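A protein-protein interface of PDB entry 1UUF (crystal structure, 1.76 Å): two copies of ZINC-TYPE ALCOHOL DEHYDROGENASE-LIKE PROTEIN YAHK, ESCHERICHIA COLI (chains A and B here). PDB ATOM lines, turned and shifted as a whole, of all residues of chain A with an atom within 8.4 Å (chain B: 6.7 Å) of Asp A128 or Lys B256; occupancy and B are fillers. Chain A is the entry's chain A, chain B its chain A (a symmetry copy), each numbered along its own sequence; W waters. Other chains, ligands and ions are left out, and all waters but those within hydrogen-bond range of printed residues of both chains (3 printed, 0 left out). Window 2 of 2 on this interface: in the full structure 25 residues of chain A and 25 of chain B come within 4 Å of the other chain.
OD1 of Asp A128 lies within salt-bridge range of NZ of Lys B256, at 2.8 Å. OD1 of Asp A128 is in salt-bridge range of NZ of Lys B305 (2.6 Å). The side-chain carboxylate of Glu A118 is in salt-bridge range of the guanidinium group of Arg B280, 3.0 Å away. The guanidinium group (NH2) of Arg B280 lies within salt-bridge range of the side-chain carboxylate (OE2) of Glu A117. O of Tyr A126 is in hydrogen-bond range of NZ of Lys B305, 2.7 Å away.
The backbone NH of Lys B256 lies within hydrogen-bond range of the backbone carbonyl oxygen of Thr B276, 2.9 Å away. The side-chain amide oxygen (OD1) of Asn A125 lies close to the backbone carbonyl oxygen (O) of Leu A123 (3.4 Å). The backbone carbonyl oxygen (O) of Glu A118 is in hydrogen-bond range of the backbone NH (N) of Leu A123, 2.8 Å away. SG of Cys A116 sits close to N of Glu A118 (3.5 Å).
Among the printed residues, pairs that only touch across the chains: Leu A123 with Arg B280 (3.5 Å).
Of the printed residues of chain B, Glu A117 touches Arg B280. Printed residues of chain B within 4 Å of Tyr A126: Lys B305 (2.7 Å). Of chain A, only Asp A128 (2.8 Å) comes within 4 Å of Lys B256. Of the printed residues of chain A, Lys B305 touches Tyr A126 and Asp A128. The nearest residue of chain A that does not touch Lys B256 is Tyr A126 (6.9 Å).
Of the 16 printed residues of chain A, 5 touch a printed residue of chain B. Among the printed residues, 6 pairs touch across the chains. Among the printed residues, Asp or Glu carboxylates within 4 Å of a Lys or Arg side-chain nitrogen of the other chain: Glu A117 with Arg B280 (3.7 Å), Glu A118 with Arg B280 (3.0 Å), Asp A128 with Lys B256 (2.8 Å) and Asp A128 with Lys B305 (2.6 Å).
No position is printed for both chains.
Water W1 lies within hydrogen-bond range of OE1 of Glu A117 (2.7 Å) and NZ of Lys B279 (2.7 Å). Water W2 bridges O of Arg B280 (2.9 Å) and OE2 of Glu A117 (3.5 Å). Water W3 bridges NZ of Lys B305 (2.9 Å) and OE1 of Glu A118 (3.0 Å).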
ATOM      1  N   ASP A 111       4.487 -15.667  -5.854  1.00  0.00           N
ATOM      2  CA  ASP A 111       4.533 -16.655  -6.933  1.00  0.00           C
ATOM      3  C   ASP A 111       3.194 -16.739  -7.667  1.00  0.00           C
ATOM      4  O   ASP A 111       2.174 -16.253  -7.180  1.00  0.00           O
ATOM      5  CB  ASP A 111       4.907 -18.043  -6.385  1.00  0.00           C
ATOM      6  CG  ASP A 111       5.704 -18.879  -7.385  1.00  0.00           C
ATOM      7  OD1 ASP A 111       5.840 -18.456  -8.554  1.00  0.00           O
ATOM      8  OD2 ASP A 111       6.197 -19.965  -7.002  1.00  0.00           O
ATOM      9  N   SER A 112       3.213 -17.320  -8.861  1.00  0.00           N
ATOM     10  CA  SER A 112       1.998 -17.508  -9.650  1.00  0.00           C
ATOM     11  C   SER A 112       2.263 -18.664 -10.616  1.00  0.00           C
ATOM     12  O   SER A 112       3.393 -19.148 -10.704  1.00  0.00           O
ATOM     13  CB  SER A 112       1.614 -16.228 -10.404  1.00  0.00           C
ATOM     14  OG  SER A 112       2.567 -15.873 -11.387  1.00  0.00           O
ATOM     15  N   CYS A 113       1.242 -19.114 -11.335  1.00  0.00           N
ATOM     16  CA  CYS A 113       1.432 -20.251 -12.236  1.00  0.00           C
ATOM     17  C   CYS A 113       2.375 -19.966 -13.405  1.00  0.00           C
ATOM     18  O   CYS A 113       3.032 -20.874 -13.907  1.00  0.00           O
ATOM     19  CB  CYS A 113       0.078 -20.771 -12.738  1.00  0.00           C
ATOM     20  SG  CYS A 113      -0.598 -20.001 -14.221  1.00  0.00           S
ATOM     21  N   CYS A 116      -0.740 -18.945 -17.421  1.00  0.00           N
ATOM     22  CA  CYS A 116      -2.126 -18.651 -17.776  1.00  0.00           C
ATOM     23  C   CYS A 116      -2.174 -17.294 -18.473  1.00  0.00           C
ATOM     24  O   CYS A 116      -1.177 -16.572 -18.511  1.00  0.00           O
ATOM     25  CB  CYS A 116      -3.015 -18.620 -16.529  1.00  0.00           C
ATOM     26  SG  CYS A 116      -2.756 -17.176 -15.476  1.00  0.00           S
ATOM     27  N   GLU A 117      -3.333 -16.944 -19.020  1.00  0.00           N
ATOM     28  CA  GLU A 117      -3.479 -15.677 -19.719  1.00  0.00           C
ATOM     29  C   GLU A 117      -3.095 -14.481 -18.846  1.00  0.00           C
ATOM     30  O   GLU A 117      -2.429 -13.555 -19.309  1.00  0.00           O
ATOM     31  CB  GLU A 117      -4.915 -15.512 -20.218  1.00  0.00           C
ATOM     32  CG  GLU A 117      -5.110 -14.308 -21.126  1.00  0.00           C
ATOM     33  CD  GLU A 117      -6.524 -14.213 -21.669  1.00  0.00           C
ATOM     34  OE1 GLU A 117      -7.003 -15.205 -22.260  1.00  0.00           O
ATOM     35  OE2 GLU A 117      -7.155 -13.149 -21.508  1.00  0.00           O
ATOM     36  N   GLU A 118      -3.509 -14.503 -17.584  1.00  0.00           N
ATOM     37  CA  GLU A 118      -3.201 -13.408 -16.668  1.00  0.00           C
ATOM     38  C   GLU A 118      -1.701 -13.243 -16.433  1.00  0.00           C
ATOM     39  O   GLU A 118      -1.162 -12.151 -16.569  1.00  0.00           O
ATOM     40  CB  GLU A 118      -3.923 -13.621 -15.333  1.00  0.00           C
ATOM     41  CG  GLU A 118      -5.406 -13.257 -15.366  1.00  0.00           C
ATOM     42  CD  GLU A 118      -6.190 -14.033 -16.412  1.00  0.00           C
ATOM     43  OE1 GLU A 118      -6.301 -15.272 -16.283  1.00  0.00           O
ATOM     44  OE2 GLU A 118      -6.693 -13.400 -17.363  1.00  0.00           O
ATOM     45  N   CYS A 119      -1.025 -14.331 -16.085  1.00  0.00           N
ATOM     46  CA  CYS A 119       0.411 -14.271 -15.842  1.00  0.00           C
ATOM     47  C   CYS A 119       1.177 -13.825 -17.083  1.00  0.00           C
ATOM     48  O   CYS A 119       2.110 -13.029 -16.993  1.00  0.00           O
ATOM     49  CB  CYS A 119       0.924 -15.634 -15.372  1.00  0.00           C
ATOM     50  SG  CYS A 119       0.447 -16.042 -13.676  1.00  0.00           S
ATOM     51  N   LEU A 123      -0.232  -9.873 -15.331  1.00  0.00           N
ATOM     52  CA  LEU A 123      -1.268  -9.682 -14.324  1.00  0.00           C
ATOM     53  C   LEU A 123      -1.283 -10.866 -13.360  1.00  0.00           C
ATOM     54  O   LEU A 123      -2.313 -11.506 -13.153  1.00  0.00           O
ATOM     55  CB  LEU A 123      -2.638  -9.529 -14.999  1.00  0.00           C
ATOM     56  CG  LEU A 123      -2.795  -8.296 -15.890  1.00  0.00           C
ATOM     57  CD1 LEU A 123      -4.137  -8.348 -16.601  1.00  0.00           C
ATOM     58  CD2 LEU A 123      -2.682  -7.027 -15.049  1.00  0.00           C
ATOM     59  N   GLU A 124      -0.128 -11.154 -12.771  1.00  0.00           N
ATOM     60  CA  GLU A 124      -0.014 -12.266 -11.835  1.00  0.00           C
ATOM     61  C   GLU A 124      -0.982 -12.113 -10.665  1.00  0.00           C
ATOM     62  O   GLU A 124      -1.336 -13.096 -10.015  1.00  0.00           O
ATOM     63  CB  GLU A 124       1.422 -12.373 -11.317  1.00  0.00           C
ATOM     64  CG  GLU A 124       2.445 -12.617 -12.416  1.00  0.00           C
ATOM     65  CD  GLU A 124       3.077 -11.340 -12.955  1.00  0.00           C
ATOM     66  OE1 GLU A 124       2.480 -10.248 -12.821  1.00  0.00           O
ATOM     67  OE2 GLU A 124       4.178 -11.439 -13.534  1.00  0.00           O
ATOM     68  N   ASN A 125      -1.413 -10.879 -10.408  1.00  0.00           N
ATOM     69  CA  ASN A 125      -2.347 -10.599  -9.319  1.00  0.00           C
ATOM     70  C   ASN A 125      -3.737 -11.196  -9.558  1.00  0.00           C
ATOM     71  O   ASN A 125      -4.489 -11.439  -8.610  1.00  0.00           O
ATOM     72  CB  ASN A 125      -2.453  -9.082  -9.092  1.00  0.00           C
ATOM     73  CG  ASN A 125      -2.813  -8.312 -10.360  1.00  0.00           C
ATOM     74  OD1 ASN A 125      -2.281  -8.575 -11.438  1.00  0.00           O
ATOM     75  ND2 ASN A 125      -3.704  -7.331 -10.223  1.00  0.00           N
ATOM     76  N   TYR A 126      -4.071 -11.437 -10.823  1.00  0.00           N
ATOM     77  CA  TYR A 126      -5.365 -12.011 -11.167  1.00  0.00           C
ATOM     78  C   TYR A 126      -5.272 -13.495 -11.516  1.00  0.00           C
ATOM     79  O   TYR A 126      -6.234 -14.095 -11.991  1.00  0.00           O
ATOM     80  CB  TYR A 126      -5.996 -11.229 -12.323  1.00  0.00           C
ATOM     81  CG  TYR A 126      -6.377  -9.818 -11.927  1.00  0.00           C
ATOM     82  CD1 TYR A 126      -5.871  -8.714 -12.612  1.00  0.00           C
ATOM     83  CD2 TYR A 126      -7.213  -9.587 -10.834  1.00  0.00           C
ATOM     84  CE1 TYR A 126      -6.182  -7.412 -12.213  1.00  0.00           C
ATOM     85  CE2 TYR A 126      -7.531  -8.295 -10.424  1.00  0.00           C
ATOM     86  CZ  TYR A 126      -7.009  -7.213 -11.113  1.00  0.00           C
ATOM     87  OH  TYR A 126      -7.289  -5.942 -10.674  1.00  0.00           O
ATOM     88  N   CYS A 127      -4.106 -14.086 -11.281  1.00  0.00           N
ATOM     89  CA  CYS A 127      -3.910 -15.507 -11.551  1.00  0.00           C
ATOM     90  C   CYS A 127      -4.763 -16.307 -10.565  1.00  0.00           C
ATOM     91  O   CYS A 127      -4.830 -15.968  -9.384  1.00  0.00           O
ATOM     92  CB  CYS A 127      -2.429 -15.872 -11.377  1.00  0.00           C
ATOM     93  SG  CYS A 127      -2.046 -17.646 -11.474  1.00  0.00           S
ATOM     94  N   ASP A 128      -5.423 -17.359 -11.042  1.00  0.00           N
ATOM     95  CA  ASP A 128      -6.254 -18.180 -10.161  1.00  0.00           C
ATOM     96  C   ASP A 128      -5.421 -18.958  -9.160  1.00  0.00           C
ATOM     97  O   ASP A 128      -5.941 -19.443  -8.152  1.00  0.00           O
ATOM     98  CB  ASP A 128      -7.082 -19.189 -10.959  1.00  0.00           C
ATOM     99  CG  ASP A 128      -8.319 -18.577 -11.571  1.00  0.00           C
ATOM    100  OD1 ASP A 128      -8.912 -17.676 -10.942  1.00  0.00           O
ATOM    101  OD2 ASP A 128      -8.710 -19.019 -12.672  1.00  0.00           O
ATOM    102  N   HIS A 129      -4.131 -19.087  -9.438  1.00  0.00           N
ATOM    103  CA  HIS A 129      -3.252 -19.847  -8.562  1.00  0.00           C
ATOM    104  C   HIS A 129      -2.105 -19.006  -8.036  1.00  0.00           C
ATOM    105  O   HIS A 129      -0.995 -19.494  -7.847  1.00  0.00           O
ATOM    106  CB  HIS A 129      -2.729 -21.061  -9.321  1.00  0.00           C
ATOM    107  CG  HIS A 129      -3.811 -21.840  -9.995  1.00  0.00           C
ATOM    108  ND1 HIS A 129      -4.763 -22.547  -9.294  1.00  0.00           N
ATOM    109  CD2 HIS A 129      -4.142 -21.961 -11.303  1.00  0.00           C
ATOM    110  CE1 HIS A 129      -5.634 -23.067 -10.139  1.00  0.00           C
ATOM    111  NE2 HIS A 129      -5.281 -22.725 -11.364  1.00  0.00           N
ATOM    112  N   MET A 130      -2.388 -17.733  -7.799  1.00  0.00           N
ATOM    113  CA  MET A 130      -1.383 -16.823  -7.285  1.00  0.00           C
ATOM    114  C   MET A 130      -1.064 -17.184  -5.836  1.00  0.00           C
ATOM    115  O   MET A 130      -1.966 -17.485  -5.049  1.00  0.00           O
ATOM    116  CB  MET A 130      -1.894 -15.383  -7.380  1.00  0.00           C
ATOM    117  CG  MET A 130      -0.919 -14.326  -6.895  1.00  0.00           C
ATOM    118  SD  MET A 130      -1.190 -13.871  -5.176  1.00  0.00           S
ATOM    119  CE  MET A 130      -2.510 -12.683  -5.386  1.00  0.00           C
ATOM    120  N   THR A 131       0.221 -17.175  -5.498  1.00  0.00           N
ATOM    121  CA  THR A 131       0.658 -17.478  -4.140  1.00  0.00           C
ATOM    122  C   THR A 131       0.854 -16.158  -3.405  1.00  0.00           C
ATOM    123  O   THR A 131       1.740 -15.376  -3.748  1.00  0.00           O
ATOM    124  CB  THR A 131       1.997 -18.246  -4.130  1.00  0.00           C
ATOM    125  OG1 THR A 131       1.835 -19.504  -4.799  1.00  0.00           O
ATOM    126  CG2 THR A 131       2.459 -18.501  -2.693  1.00  0.00           C
ATOM    127  N   ALA B 252     -22.331 -23.404 -12.285  1.00  0.00           N
ATOM    128  CA  ALA B 252     -20.936 -23.694 -11.972  1.00  0.00           C
ATOM    129  C   ALA B 252     -20.113 -24.112 -13.186  1.00  0.00           C
ATOM    130  O   ALA B 252     -18.905 -23.875 -13.237  1.00  0.00           O
ATOM    131  CB  ALA B 252     -20.862 -24.776 -10.898  1.00  0.00           C
ATOM    132  N   HIS B 254     -20.000 -22.802 -15.916  1.00  0.00           N
ATOM    133  CA  HIS B 254     -19.594 -21.625 -16.685  1.00  0.00           C
ATOM    134  C   HIS B 254     -18.811 -20.607 -15.868  1.00  0.00           C
ATOM    135  O   HIS B 254     -18.689 -19.444 -16.256  1.00  0.00           O
ATOM    136  CB  HIS B 254     -20.832 -20.952 -17.281  1.00  0.00           C
ATOM    137  CG  HIS B 254     -21.585 -21.823 -18.238  1.00  0.00           C
ATOM    138  ND1 HIS B 254     -21.231 -21.950 -19.564  1.00  0.00           N
ATOM    139  CD2 HIS B 254     -22.655 -22.631 -18.055  1.00  0.00           C
ATOM    140  CE1 HIS B 254     -22.050 -22.801 -20.156  1.00  0.00           C
ATOM    141  NE2 HIS B 254     -22.923 -23.229 -19.262  1.00  0.00           N
ATOM    142  N   LEU B 255     -18.280 -21.042 -14.734  1.00  0.00           N
ATOM    143  CA  LEU B 255     -17.507 -20.159 -13.869  1.00  0.00           C
ATOM    144  C   LEU B 255     -16.388 -19.448 -14.632  1.00  0.00           C
ATOM    145  O   LEU B 255     -15.689 -20.064 -15.440  1.00  0.00           O
ATOM    146  CB  LEU B 255     -16.894 -20.962 -12.719  1.00  0.00           C
ATOM    147  CG  LEU B 255     -16.071 -20.173 -11.700  1.00  0.00           C
ATOM    148  CD1 LEU B 255     -17.001 -19.347 -10.816  1.00  0.00           C
ATOM    149  CD2 LEU B 255     -15.257 -21.136 -10.851  1.00  0.00           C
ATOM    150  N   LYS B 256     -16.230 -18.152 -14.371  1.00  0.00           N
ATOM    151  CA  LYS B 256     -15.186 -17.337 -14.995  1.00  0.00           C
ATOM    152  C   LYS B 256     -14.978 -17.632 -16.481  1.00  0.00           C
ATOM    153  O   LYS B 256     -13.844 -17.823 -16.918  1.00  0.00           O
ATOM    154  CB  LYS B 256     -13.858 -17.557 -14.259  1.00  0.00           C
ATOM    155  CG  LYS B 256     -13.922 -17.322 -12.758  1.00  0.00           C
ATOM    156  CD  LYS B 256     -12.626 -17.751 -12.075  1.00  0.00           C
ATOM    157  CE  LYS B 256     -12.691 -17.552 -10.565  1.00  0.00           C
ATOM    158  NZ  LYS B 256     -11.464 -18.046  -9.868  1.00  0.00           N
ATOM    159  N   SER B 257     -16.050 -17.641 -17.269  1.00  0.00           N
ATOM    160  CA  SER B 257     -15.907 -17.954 -18.688  1.00  0.00           C
ATOM    161  C   SER B 257     -16.500 -16.948 -19.664  1.00  0.00           C
ATOM    162  O   SER B 257     -16.249 -17.039 -20.870  1.00  0.00           O
ATOM    163  CB  SER B 257     -16.532 -19.320 -18.982  1.00  0.00           C
ATOM    164  OG  SER B 257     -17.943 -19.252 -18.868  1.00  0.00           O
ATOM    165  N   PHE B 258     -17.282 -15.995 -19.164  1.00  0.00           N
ATOM    166  CA  PHE B 258     -17.911 -15.018 -20.049  1.00  0.00           C
ATOM    167  C   PHE B 258     -17.149 -13.726 -20.268  1.00  0.00           C
ATOM    168  O   PHE B 258     -16.622 -13.131 -19.335  1.00  0.00           O
ATOM    169  CB  PHE B 258     -19.311 -14.659 -19.550  1.00  0.00           C
ATOM    170  CG  PHE B 258     -20.328 -15.733 -19.772  1.00  0.00           C
ATOM    171  CD1 PHE B 258     -20.533 -16.721 -18.818  1.00  0.00           C
ATOM    172  CD2 PHE B 258     -21.075 -15.763 -20.944  1.00  0.00           C
ATOM    173  CE1 PHE B 258     -21.470 -17.728 -19.026  1.00  0.00           C
ATOM    174  CE2 PHE B 258     -22.014 -16.763 -21.165  1.00  0.00           C
ATOM    175  CZ  PHE B 258     -22.213 -17.749 -20.200  1.00  0.00           C
ATOM    176  N   THR B 275     -21.968 -12.510 -11.719  1.00  0.00           N
ATOM    177  CA  THR B 275     -20.677 -11.835 -11.683  1.00  0.00           C
ATOM    178  C   THR B 275     -19.544 -12.859 -11.662  1.00  0.00           C
ATOM    179  O   THR B 275     -18.515 -12.673 -12.311  1.00  0.00           O
ATOM    180  CB  THR B 275     -20.575 -10.913 -10.453  1.00  0.00           C
ATOM    181  OG1 THR B 275     -21.569  -9.884 -10.557  1.00  0.00           O
ATOM    182  CG2 THR B 275     -19.198 -10.266 -10.378  1.00  0.00           C
ATOM    183  N   THR B 276     -19.740 -13.959 -10.942  1.00  0.00           N
ATOM    184  CA  THR B 276     -18.705 -14.983 -10.867  1.00  0.00           C
ATOM    185  C   THR B 276     -18.528 -15.739 -12.179  1.00  0.00           C
ATOM    186  O   THR B 276     -17.557 -16.474 -12.342  1.00  0.00           O
ATOM    187  CB  THR B 276     -18.993 -16.002  -9.746  1.00  0.00           C
ATOM    188  OG1 THR B 276     -20.187 -16.729 -10.052  1.00  0.00           O
ATOM    189  CG2 THR B 276     -19.165 -15.290  -8.420  1.00  0.00           C
ATOM    190  N   LEU B 277     -19.459 -15.554 -13.116  1.00  0.00           N
ATOM    191  CA  LEU B 277     -19.377 -16.222 -14.417  1.00  0.00           C
ATOM    192  C   LEU B 277     -18.545 -15.405 -15.411  1.00  0.00           C
ATOM    193  O   LEU B 277     -18.243 -15.868 -16.512  1.00  0.00           O
ATOM    194  CB  LEU B 277     -20.775 -16.431 -15.006  1.00  0.00           C
ATOM    195  CG  LEU B 277     -21.826 -17.125 -14.140  1.00  0.00           C
ATOM    196  CD1 LEU B 277     -23.079 -17.351 -14.976  1.00  0.00           C
ATOM    197  CD2 LEU B 277     -21.287 -18.447 -13.613  1.00  0.00           C
ATOM    198  N   LEU B 278     -18.183 -14.186 -15.021  1.00  0.00           N
ATOM    199  CA  LEU B 278     -17.394 -13.304 -15.880  1.00  0.00           C
ATOM    200  C   LEU B 278     -15.894 -13.561 -15.814  1.00  0.00           C
ATOM    201  O   LEU B 278     -15.353 -13.830 -14.748  1.00  0.00           O
ATOM    202  CB  LEU B 278     -17.632 -11.845 -15.494  1.00  0.00           C
ATOM    203  CG  LEU B 278     -19.027 -11.255 -15.673  1.00  0.00           C
ATOM    204  CD1 LEU B 278     -19.067  -9.876 -15.017  1.00  0.00           C
ATOM    205  CD2 LEU B 278     -19.360 -11.165 -17.154  1.00  0.00           C
ATOM    206  N   LYS B 279     -15.228 -13.458 -16.961  1.00  0.00           N
ATOM    207  CA  LYS B 279     -13.778 -13.629 -17.016  1.00  0.00           C
ATOM    208  C   LYS B 279     -13.176 -12.364 -16.424  1.00  0.00           C
ATOM    209  O   LYS B 279     -13.888 -11.399 -16.144  1.00  0.00           O
ATOM    210  CB  LYS B 279     -13.301 -13.744 -18.463  1.00  0.00           C
ATOM    211  CG  LYS B 279     -13.773 -14.983 -19.197  1.00  0.00           C
ATOM    212  CD  LYS B 279     -13.532 -14.848 -20.693  1.00  0.00           C
ATOM    213  CE  LYS B 279     -12.059 -14.626 -21.015  1.00  0.00           C
ATOM    214  NZ  LYS B 279     -11.846 -14.525 -22.487  1.00  0.00           N
ATOM    215  N   ARG B 280     -11.861 -12.373 -16.234  1.00  0.00           N
ATOM    216  CA  ARG B 280     -11.164 -11.205 -15.722  1.00  0.00           C
ATOM    217  C   ARG B 280     -11.421 -10.088 -16.729  1.00  0.00           C
ATOM    218  O   ARG B 280     -11.383 -10.318 -17.941  1.00  0.00           O
ATOM    219  CB  ARG B 280      -9.663 -11.502 -15.613  1.00  0.00           C
ATOM    220  CG  ARG B 280      -8.803 -10.314 -15.187  1.00  0.00           C
ATOM    221  CD  ARG B 280      -8.228  -9.586 -16.391  1.00  0.00           C
ATOM    222  NE  ARG B 280      -7.317 -10.436 -17.153  1.00  0.00           N
ATOM    223  CZ  ARG B 280      -6.709 -10.067 -18.275  1.00  0.00           C
ATOM    224  NH1 ARG B 280      -6.910  -8.855 -18.775  1.00  0.00           N
ATOM    225  NH2 ARG B 280      -5.905 -10.915 -18.902  1.00  0.00           N
ATOM    226  N   LYS B 305     -11.353 -10.042  -9.813  1.00  0.00           N
ATOM    227  CA  LYS B 305     -11.058 -10.234 -11.231  1.00  0.00           C
ATOM    228  C   LYS B 305     -11.233  -8.978 -12.070  1.00  0.00           C
ATOM    229  O   LYS B 305     -11.324  -9.060 -13.294  1.00  0.00           O
ATOM    230  CB  LYS B 305     -11.949 -11.341 -11.805  1.00  0.00           C
ATOM    231  CG  LYS B 305     -11.653 -12.732 -11.258  1.00  0.00           C
ATOM    232  CD  LYS B 305     -10.302 -13.234 -11.738  1.00  0.00           C
ATOM    233  CE  LYS B 305     -10.072 -14.674 -11.303  1.00  0.00           C
ATOM    234  NZ  LYS B 305      -8.724 -15.152 -11.711  1.00  0.00           N
ATOM    235  N   ARG B 307     -13.770  -7.046 -12.502  1.00  0.00           N
ATOM    236  CA  ARG B 307     -15.000  -7.158 -13.274  1.00  0.00           C
ATOM    237  C   ARG B 307     -15.808  -5.896 -13.055  1.00  0.00           C
ATOM    238  O   ARG B 307     -15.512  -5.109 -12.157  1.00  0.00           O
ATOM    239  CB  ARG B 307     -15.816  -8.348 -12.793  1.00  0.00           C
ATOM    240  CG  ARG B 307     -15.195  -9.697 -13.067  1.00  0.00           C
ATOM    241  CD  ARG B 307     -15.727 -10.689 -12.056  1.00  0.00           C
ATOM    242  NE  ARG B 307     -15.424 -12.074 -12.391  1.00  0.00           N
ATOM    243  CZ  ARG B 307     -15.328 -13.044 -11.490  1.00  0.00           C
ATOM    244  NH1 ARG B 307     -15.499 -12.769 -10.203  1.00  0.00           N
ATOM    245  NH2 ARG B 307     -15.079 -14.287 -11.874  1.00  0.00           N
HETATM  246  O   HOH W   1      -9.258 -14.130 -23.206  1.00  0.00           O
HETATM  247  O   HOH W   2      -9.882 -11.939 -19.749  1.00  0.00           O
HETATM  248  O   HOH W   3      -8.816 -15.075 -14.615  1.00  0.00           O
